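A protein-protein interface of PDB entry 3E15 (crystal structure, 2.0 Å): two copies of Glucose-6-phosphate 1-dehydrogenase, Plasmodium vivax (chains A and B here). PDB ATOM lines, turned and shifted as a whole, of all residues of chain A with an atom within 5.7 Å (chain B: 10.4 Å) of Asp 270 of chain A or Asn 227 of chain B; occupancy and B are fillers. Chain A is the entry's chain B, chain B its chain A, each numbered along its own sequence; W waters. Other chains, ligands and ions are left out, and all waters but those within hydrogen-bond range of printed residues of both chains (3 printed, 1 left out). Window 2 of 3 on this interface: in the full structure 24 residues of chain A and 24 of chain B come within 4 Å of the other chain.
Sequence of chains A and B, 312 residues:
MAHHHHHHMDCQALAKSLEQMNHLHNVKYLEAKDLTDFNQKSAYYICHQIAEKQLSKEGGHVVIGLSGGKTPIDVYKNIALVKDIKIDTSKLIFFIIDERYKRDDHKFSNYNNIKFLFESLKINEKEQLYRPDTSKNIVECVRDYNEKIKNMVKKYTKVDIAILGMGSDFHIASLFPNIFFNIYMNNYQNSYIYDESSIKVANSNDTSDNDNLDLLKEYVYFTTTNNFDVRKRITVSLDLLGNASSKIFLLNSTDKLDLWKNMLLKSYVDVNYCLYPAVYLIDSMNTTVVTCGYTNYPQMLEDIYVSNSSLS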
ATOM      1  N   LYS A 266     -27.261  29.075  17.981  1.00  0.00           N
ATOM      2  CA  LYS A 266     -26.538  27.848  18.241  1.00  0.00           C
ATOM      3  C   LYS A 266     -25.128  28.137  18.710  1.00  0.00           C
ATOM      4  O   LYS A 266     -24.498  27.285  19.331  1.00  0.00           O
ATOM      5  CB  LYS A 266     -26.520  27.000  16.974  1.00  0.00           C
ATOM      6  CG  LYS A 266     -27.878  26.458  16.640  1.00  0.00           C
ATOM      7  CD  LYS A 266     -27.865  25.637  15.336  1.00  0.00           C
ATOM      8  CE  LYS A 266     -27.924  24.168  15.568  1.00  0.00           C
ATOM      9  NZ  LYS A 266     -28.325  23.266  14.354  1.00  0.00           N
ATOM     10  N   SER A 267     -24.631  29.338  18.390  1.00  0.00           N
ATOM     11  CA  SER A 267     -23.284  29.741  18.734  1.00  0.00           C
ATOM     12  C   SER A 267     -23.226  30.556  20.031  1.00  0.00           C
ATOM     13  O   SER A 267     -22.160  30.944  20.463  1.00  0.00           O
ATOM     14  CB  SER A 267     -22.642  30.530  17.573  1.00  0.00           C
ATOM     15  OG  SER A 267     -23.212  31.825  17.454  1.00  0.00           O
ATOM     16  N   TYR A 268     -24.369  30.785  20.660  1.00  0.00           N
ATOM     17  CA  TYR A 268     -24.414  31.542  21.927  1.00  0.00           C
ATOM     18  C   TYR A 268     -23.526  30.925  23.031  1.00  0.00           C
ATOM     19  O   TYR A 268     -22.915  31.638  23.816  1.00  0.00           O
ATOM     20  CB  TYR A 268     -25.861  31.635  22.417  1.00  0.00           C
ATOM     21  CG  TYR A 268     -26.056  32.529  23.628  1.00  0.00           C
ATOM     22  CD1 TYR A 268     -25.726  33.882  23.578  1.00  0.00           C
ATOM     23  CD2 TYR A 268     -26.587  32.027  24.814  1.00  0.00           C
ATOM     24  CE1 TYR A 268     -25.901  34.705  24.672  1.00  0.00           C
ATOM     25  CE2 TYR A 268     -26.769  32.865  25.922  1.00  0.00           C
ATOM     26  CZ  TYR A 268     -26.427  34.193  25.834  1.00  0.00           C
ATOM     27  OH  TYR A 268     -26.601  35.039  26.909  1.00  0.00           O
ATOM     28  N   VAL A 269     -23.488  29.606  23.084  1.00  0.00           N
ATOM     29  CA  VAL A 269     -22.628  28.867  23.990  1.00  0.00           C
ATOM     30  C   VAL A 269     -21.540  28.066  23.255  1.00  0.00           C
ATOM     31  O   VAL A 269     -21.840  27.251  22.382  1.00  0.00           O
ATOM     32  CB  VAL A 269     -23.458  27.884  24.853  1.00  0.00           C
ATOM     33  CG1 VAL A 269     -22.515  27.063  25.807  1.00  0.00           C
ATOM     34  CG2 VAL A 269     -24.522  28.641  25.650  1.00  0.00           C
ATOM     35  N   ASP A 270     -20.289  28.303  23.636  1.00  0.00           N
ATOM     36  CA  ASP A 270     -19.122  27.541  23.155  1.00  0.00           C
ATOM     37  C   ASP A 270     -19.041  27.493  21.636  1.00  0.00           C
ATOM     38  O   ASP A 270     -18.880  26.418  21.045  1.00  0.00           O
ATOM     39  CB  ASP A 270     -19.113  26.123  23.717  1.00  0.00           C
ATOM     40  CG  ASP A 270     -18.764  26.087  25.194  1.00  0.00           C
ATOM     41  OD1 ASP A 270     -17.956  26.926  25.625  1.00  0.00           O
ATOM     42  OD2 ASP A 270     -19.300  25.229  25.903  1.00  0.00           O
ATOM     43  N   VAL A 271     -19.129  28.661  21.009  1.00  0.00           N
ATOM     44  CA  VAL A 271     -19.024  28.757  19.545  1.00  0.00           C
ATOM     45  C   VAL A 271     -17.766  28.043  19.056  1.00  0.00           C
ATOM     46  O   VAL A 271     -16.675  28.272  19.557  1.00  0.00           O
ATOM     47  CB  VAL A 271     -19.048  30.230  19.056  1.00  0.00           C
ATOM     48  CG1 VAL A 271     -17.924  31.034  19.643  1.00  0.00           C
ATOM     49  CG2 VAL A 271     -19.032  30.308  17.517  1.00  0.00           C
ATOM     50  N   ASN A 272     -17.946  27.169  18.065  1.00  0.00           N
ATOM     51  CA  ASN A 272     -16.845  26.617  17.289  1.00  0.00           C
ATOM     52  C   ASN A 272     -16.680  27.453  15.994  1.00  0.00           C
ATOM     53  O   ASN A 272     -17.512  27.389  15.082  1.00  0.00           O
ATOM     54  CB  ASN A 272     -17.115  25.111  16.980  1.00  0.00           C
ATOM     55  CG  ASN A 272     -15.929  24.408  16.333  1.00  0.00           C
ATOM     56  OD1 ASN A 272     -15.015  25.056  15.783  1.00  0.00           O
ATOM     57  ND2 ASN A 272     -15.928  23.062  16.388  1.00  0.00           N
ATOM     58  N   LEU A 275     -16.951  25.917  12.575  1.00  0.00           N
ATOM     59  CA  LEU A 275     -18.272  25.592  12.095  1.00  0.00           C
ATOM     60  C   LEU A 275     -19.133  26.821  11.832  1.00  0.00           C
ATOM     61  O   LEU A 275     -20.051  26.766  11.002  1.00  0.00           O
ATOM     62  CB  LEU A 275     -18.956  24.659  13.087  1.00  0.00           C
ATOM     63  CG  LEU A 275     -18.194  23.355  13.379  1.00  0.00           C
ATOM     64  CD1 LEU A 275     -18.935  22.559  14.505  1.00  0.00           C
ATOM     65  CD2 LEU A 275     -18.090  22.524  12.108  1.00  0.00           C
ATOM     66  N   ARG B 100     -25.542  10.807  20.665  1.00  0.00           N
ATOM     67  CA  ARG B 100     -25.011  12.085  21.133  1.00  0.00           C
ATOM     68  C   ARG B 100     -24.361  11.892  22.485  1.00  0.00           C
ATOM     69  O   ARG B 100     -25.032  11.636  23.469  1.00  0.00           O
ATOM     70  CB  ARG B 100     -26.163  13.113  21.222  1.00  0.00           C
ATOM     71  CG  ARG B 100     -26.873  13.215  19.923  1.00  0.00           C
ATOM     72  CD  ARG B 100     -27.963  14.242  19.867  1.00  0.00           C
ATOM     73  NE  ARG B 100     -28.541  14.194  18.511  1.00  0.00           N
ATOM     74  CZ  ARG B 100     -29.025  15.247  17.841  1.00  0.00           C
ATOM     75  NH1 ARG B 100     -29.048  16.462  18.404  1.00  0.00           N
ATOM     76  NH2 ARG B 100     -29.511  15.076  16.600  1.00  0.00           N
ATOM     77  N   TYR B 101     -23.044  12.019  22.525  1.00  0.00           N
ATOM     78  CA  TYR B 101     -22.274  11.597  23.664  1.00  0.00           C
ATOM     79  C   TYR B 101     -22.216  12.704  24.708  1.00  0.00           C
ATOM     80  O   TYR B 101     -21.813  13.823  24.423  1.00  0.00           O
ATOM     81  CB  TYR B 101     -20.880  11.242  23.219  1.00  0.00           C
ATOM     82  CG  TYR B 101     -19.918  10.883  24.317  1.00  0.00           C
ATOM     83  CD1 TYR B 101     -19.773   9.576  24.740  1.00  0.00           C
ATOM     84  CD2 TYR B 101     -19.160  11.863  24.944  1.00  0.00           C
ATOM     85  CE1 TYR B 101     -18.868   9.248  25.743  1.00  0.00           C
ATOM     86  CE2 TYR B 101     -18.269  11.554  25.927  1.00  0.00           C
ATOM     87  CZ  TYR B 101     -18.124  10.239  26.327  1.00  0.00           C
ATOM     88  OH  TYR B 101     -17.255   9.939  27.314  1.00  0.00           O
ATOM     89  N   LYS B 102     -22.599  12.376  25.926  1.00  0.00           N
ATOM     90  CA  LYS B 102     -22.369  13.258  27.062  1.00  0.00           C
ATOM     91  C   LYS B 102     -22.079  12.376  28.251  1.00  0.00           C
ATOM     92  O   LYS B 102     -22.987  11.767  28.762  1.00  0.00           O
ATOM     93  CB  LYS B 102     -23.630  14.062  27.363  1.00  0.00           C
ATOM     94  CG  LYS B 102     -23.809  15.330  26.584  1.00  0.00           C
ATOM     95  CD  LYS B 102     -25.044  16.121  27.100  1.00  0.00           C
ATOM     96  CE  LYS B 102     -26.021  16.390  25.984  1.00  0.00           C
ATOM     97  NZ  LYS B 102     -27.296  16.961  26.458  1.00  0.00           N
ATOM     98  N   PHE B 176     -21.192  13.176   9.450  1.00  0.00           N
ATOM     99  CA  PHE B 176     -21.247  14.591   9.081  1.00  0.00           C
ATOM    100  C   PHE B 176     -20.263  14.859   7.951  1.00  0.00           C
ATOM    101  O   PHE B 176     -19.095  14.543   8.076  1.00  0.00           O
ATOM    102  CB  PHE B 176     -20.878  15.477  10.296  1.00  0.00           C
ATOM    103  CG  PHE B 176     -21.970  15.553  11.310  1.00  0.00           C
ATOM    104  CD1 PHE B 176     -23.020  16.431  11.135  1.00  0.00           C
ATOM    105  CD2 PHE B 176     -21.977  14.712  12.416  1.00  0.00           C
ATOM    106  CE1 PHE B 176     -24.048  16.484  12.038  1.00  0.00           C
ATOM    107  CE2 PHE B 176     -23.016  14.769  13.328  1.00  0.00           C
ATOM    108  CZ  PHE B 176     -24.050  15.646  13.131  1.00  0.00           C
ATOM    109  N   THR B 223     -17.334  11.132  15.728  1.00  0.00           N
ATOM    110  CA  THR B 223     -17.469  12.298  14.853  1.00  0.00           C
ATOM    111  C   THR B 223     -17.892  13.490  15.644  1.00  0.00           C
ATOM    112  O   THR B 223     -18.342  13.343  16.782  1.00  0.00           O
ATOM    113  CB  THR B 223     -18.475  12.048  13.744  1.00  0.00           C
ATOM    114  OG1 THR B 223     -19.703  11.599  14.307  1.00  0.00           O
ATOM    115  CG2 THR B 223     -17.945  10.974  12.768  1.00  0.00           C
ATOM    116  N   THR B 224     -17.735  14.687  15.051  1.00  0.00           N
ATOM    117  CA  THR B 224     -18.079  15.910  15.727  1.00  0.00           C
ATOM    118  C   THR B 224     -18.945  16.840  14.893  1.00  0.00           C
ATOM    119  O   THR B 224     -18.864  16.888  13.630  1.00  0.00           O
ATOM    120  CB  THR B 224     -16.841  16.702  16.205  1.00  0.00           C
ATOM    121  OG1 THR B 224     -15.975  16.966  15.099  1.00  0.00           O
ATOM    122  CG2 THR B 224     -16.089  15.937  17.299  1.00  0.00           C
ATOM    123  N   THR B 225     -19.790  17.553  15.615  1.00  0.00           N
ATOM    124  CA  THR B 225     -20.610  18.627  15.070  1.00  0.00           C
ATOM    125  C   THR B 225     -20.585  19.832  16.024  1.00  0.00           C
ATOM    126  O   THR B 225     -19.692  19.929  16.875  1.00  0.00           O
ATOM    127  CB  THR B 225     -22.012  18.149  14.792  1.00  0.00           C
ATOM    128  OG1 THR B 225     -22.735  19.144  14.047  1.00  0.00           O
ATOM    129  CG2 THR B 225     -22.750  17.784  16.103  1.00  0.00           C
ATOM    130  N   ASN B 226     -21.544  20.750  15.889  1.00  0.00           N
ATOM    131  CA  ASN B 226     -21.530  21.955  16.722  1.00  0.00           C
ATOM    132  C   ASN B 226     -21.989  21.639  18.156  1.00  0.00           C
ATOM    133  O   ASN B 226     -22.655  20.631  18.404  1.00  0.00           O
ATOM    134  CB  ASN B 226     -22.396  23.035  16.115  1.00  0.00           C
ATOM    135  CG  ASN B 226     -23.828  22.654  16.099  1.00  0.00           C
ATOM    136  OD1 ASN B 226     -24.497  22.779  17.107  1.00  0.00           O
ATOM    137  ND2 ASN B 226     -24.318  22.120  14.948  1.00  0.00           N
ATOM    138  N   ASN B 227     -21.613  22.511  19.083  1.00  0.00           N
ATOM    139  CA  ASN B 227     -21.844  22.288  20.498  1.00  0.00           C
ATOM    140  C   ASN B 227     -23.314  22.349  20.873  1.00  0.00           C
ATOM    141  O   ASN B 227     -23.755  21.625  21.754  1.00  0.00           O
ATOM    142  CB  ASN B 227     -21.020  23.270  21.340  1.00  0.00           C
ATOM    143  CG  ASN B 227     -19.496  23.042  21.189  1.00  0.00           C
ATOM    144  OD1 ASN B 227     -18.935  23.254  20.126  1.00  0.00           O
ATOM    145  ND2 ASN B 227     -18.850  22.606  22.259  1.00  0.00           N
ATOM    146  N   PHE B 228     -24.085  23.187  20.185  1.00  0.00           N
ATOM    147  CA  PHE B 228     -25.521  23.244  20.448  1.00  0.00           C
ATOM    148  C   PHE B 228     -26.197  21.870  20.204  1.00  0.00           C
ATOM    149  O   PHE B 228     -27.068  21.473  20.956  1.00  0.00           O
ATOM    150  CB  PHE B 228     -26.187  24.302  19.580  1.00  0.00           C
ATOM    151  CG  PHE B 228     -27.669  24.503  19.877  1.00  0.00           C
ATOM    152  CD1 PHE B 228     -28.079  25.413  20.845  1.00  0.00           C
ATOM    153  CD2 PHE B 228     -28.644  23.789  19.182  1.00  0.00           C
ATOM    154  CE1 PHE B 228     -29.451  25.623  21.117  1.00  0.00           C
ATOM    155  CE2 PHE B 228     -30.026  23.984  19.457  1.00  0.00           C
ATOM    156  CZ  PHE B 228     -30.416  24.911  20.425  1.00  0.00           C
ATOM    157  N   ASP B 229     -25.777  21.162  19.153  1.00  0.00           N
ATOM    158  CA  ASP B 229     -26.406  19.902  18.753  1.00  0.00           C
ATOM    159  C   ASP B 229     -25.773  18.684  19.449  1.00  0.00           C
ATOM    160  O   ASP B 229     -26.104  17.542  19.129  1.00  0.00           O
ATOM    161  CB  ASP B 229     -26.297  19.730  17.229  1.00  0.00           C
ATOM    162  CG  ASP B 229     -27.215  20.660  16.456  1.00  0.00           C
ATOM    163  OD1 ASP B 229     -28.240  21.143  17.007  1.00  0.00           O
ATOM    164  OD2 ASP B 229     -26.902  20.904  15.267  1.00  0.00           O
ATOM    165  N   VAL B 230     -24.868  18.957  20.389  1.00  0.00           N
ATOM    166  CA  VAL B 230     -24.061  17.980  21.105  1.00  0.00           C
ATOM    167  C   VAL B 230     -22.838  17.610  20.282  1.00  0.00           C
ATOM    168  O   VAL B 230     -22.918  16.831  19.336  1.00  0.00           O
ATOM    169  CB  VAL B 230     -24.826  16.722  21.578  1.00  0.00           C
ATOM    170  CG1 VAL B 230     -23.889  15.848  22.457  1.00  0.00           C
ATOM    171  CG2 VAL B 230     -26.124  17.110  22.370  1.00  0.00           C
ATOM    172  N   ARG B 231     -21.711  18.204  20.651  1.00  0.00           N
ATOM    173  CA  ARG B 231     -20.508  18.227  19.818  1.00  0.00           C
ATOM    174  C   ARG B 231     -19.970  16.830  19.505  1.00  0.00           C
ATOM    175  O   ARG B 231     -19.615  16.558  18.363  1.00  0.00           O
ATOM    176  CB  ARG B 231     -19.427  19.068  20.487  1.00  0.00           C
ATOM    177  CG  ARG B 231     -18.018  18.810  20.013  1.00  0.00           C
ATOM    178  CD  ARG B 231     -17.011  19.539  20.877  1.00  0.00           C
ATOM    179  NE  ARG B 231     -15.653  19.084  20.613  1.00  0.00           N
ATOM    180  CZ  ARG B 231     -14.971  19.380  19.506  1.00  0.00           C
ATOM    181  NH1 ARG B 231     -15.509  20.139  18.551  1.00  0.00           N
ATOM    182  NH2 ARG B 231     -13.736  18.912  19.352  1.00  0.00           N
ATOM    183  N   LYS B 232     -19.912  15.964  20.520  1.00  0.00           N
ATOM    184  CA  LYS B 232     -19.297  14.629  20.399  1.00  0.00           C
ATOM    185  C   LYS B 232     -20.345  13.571  20.065  1.00  0.00           C
ATOM    186  O   LYS B 232     -21.354  13.463  20.757  1.00  0.00           O
ATOM    187  CB  LYS B 232     -18.583  14.264  21.690  1.00  0.00           C
ATOM    188  CG  LYS B 232     -17.411  15.158  22.040  1.00  0.00           C
ATOM    189  CD  LYS B 232     -16.602  14.530  23.165  1.00  0.00           C
ATOM    190  CE  LYS B 232     -15.629  15.496  23.797  1.00  0.00           C
ATOM    191  NZ  LYS B 232     -16.301  16.682  24.421  1.00  0.00           N
ATOM    192  N   ARG B 233     -20.097  12.815  18.989  1.00  0.00           N
ATOM    193  CA  ARG B 233     -21.002  11.790  18.487  1.00  0.00           C
ATOM    194  C   ARG B 233     -20.307  10.453  18.294  1.00  0.00           C
ATOM    195  O   ARG B 233     -19.079  10.370  18.060  1.00  0.00           O
ATOM    196  CB  ARG B 233     -21.633  12.220  17.151  1.00  0.00           C
ATOM    197  CG  ARG B 233     -22.275  13.615  17.169  1.00  0.00           C
ATOM    198  CD  ARG B 233     -23.522  13.647  18.043  1.00  0.00           C
ATOM    199  NE  ARG B 233     -24.330  14.832  17.795  1.00  0.00           N
ATOM    200  CZ  ARG B 233     -25.259  14.944  16.853  1.00  0.00           C
ATOM    201  NH1 ARG B 233     -25.530  13.941  16.024  1.00  0.00           N
ATOM    202  NH2 ARG B 233     -25.935  16.078  16.742  1.00  0.00           N
HETATM  203  O   HOH W   1     -24.156  25.497  22.323  1.00  0.00           O
HETATM  204  O   HOH W   2     -20.200  25.115  18.272  1.00  0.00           O
HETATM  205  O   HOH W   3     -18.016  21.754  18.041  1.00  0.00           O
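The side-chain carboxylate (OD2) of Asp 229 of chain B lies within salt-bridge range of the side-chain amino group (NZ) of Lys 266 of chain A, at 2.9 Å.
The backbone carbonyl oxygen (O) of Asp 270 of chain A lies close to the side-chain amide oxygen (OD1) of Asn 227 of chain B.
The side-chain amide oxygen of Asn 226 of chain B is in hydrogen-bond range of the backbone NH of Phe 228 of chain B (3.1 Å).
O of Arg 231 of chain B is in hydrogen-bond range of N of Thr 225 of chain B (2.9 Å).
The side-chain amide nitrogen (ND2) of Asn 226 of chain B lies within hydrogen-bond range of the side-chain hydroxyl (OG1) of Thr 225 of chain B (3.5 Å).
The guanidinium group (NH2) of Arg 233 of chain B sits at hydrogen-bond distance from the backbone carbonyl oxygen (O) of Asp 229 of chain B.
The backbone carbonyl oxygen (O) of Asn 226 of chain B sits at hydrogen-bond distance from the backbone NH (N) of Arg 231 of chain B, 3.4 Å away.
The side-chain amide nitrogen (ND2) of Asn 226 of chain B is in hydrogen-bond range of the side-chain carboxylate (OD2) of Asp 229 of chain B (2.9 Å).
Among the printed residues, pairs that only touch across the chains: Lys 266 of chain A with Phe 228 of chain B (3.4 Å), Leu 275 of chain A with Asn 226 of chain B (3.5 Å), Leu 275 of chain A with Thr 225 of chain B (3.5 Å) and Asn 272 of chain A with Arg 231 of chain B (3.7 Å).
Asp 270 of chain A touches just one residue of chain B: Asn 227.
Asn 227 of chain B touches just one residue of chain A: Asp 270.
No residue of chain B comes within 4 Å of Val 269 of chain A.
No residue of chain B comes within 4 Å of Val 271 of chain A.
Asn 272 of chain A touches just one residue of chain B: Arg 231 (3.7 Å).
Of the printed residues of chain A, Asp 229 of chain B touches Lys 266.
Printed residues of chain A within 4 Å of Arg 231 of chain B: Asn 272.
Printed residues of chain B within 4 Å of Lys 266 of chain A: Phe 228 and Asp 229.
Of the printed residues of chain A, Thr 225 of chain B touches Leu 275.
The nearest residue of chain A that does not touch Asn 227 of chain B is Asn 272 of chain A (4.1 Å).
The nearest printed residue of chain A that does not touch Thr 225 of chain B is Asn 272 of chain A (4.9 Å).
Of the 8 printed residues of chain A, 4 touch a printed residue of chain B.
Hydrophobic or aromatic side chains of chain A within 4 Å of the printed part of chain B: Leu 275.
Of the 15 printed residues of chain B, 6 touch a printed residue of chain A.
Hydrophobic or aromatic side chains of chain B that line the printed part of chain A: Phe 228.
Along chain B the printed residues that touch a printed residue of chain A span positions 225 to 231.
Among the printed residues, Asp or Glu carboxylates within 4 Å of a Lys or Arg side-chain nitrogen of the other chain: Lys 266 of chain A with Asp 229 of chain B (2.9 Å).
No position is printed for both chains.
Of the 6 pairs that touch across the chains among the printed residues, none has its exchanged pair printed and touching as well.
Water W3 lies within hydrogen-bond range of OD1 of Asn 227 of chain B, O of Thr 225 of chain B, ND2 of Asn 272 of chain A and NH1 of Arg 231 of chain B.
Water W1 lies within hydrogen-bond range of O of Val 269 of chain A (2.9 Å) and N of Phe 228 of chain B (3.1 Å).
Water W2 lies within hydrogen-bond range of the side-chain amide oxygen (OD1) of Asn 227 of chain B (2.9 Å), the backbone NH (N) of Asn 272 of chain A (3.1 Å) and the backbone carbonyl oxygen (O) of Asp 270 of chain A (3.3 Å).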
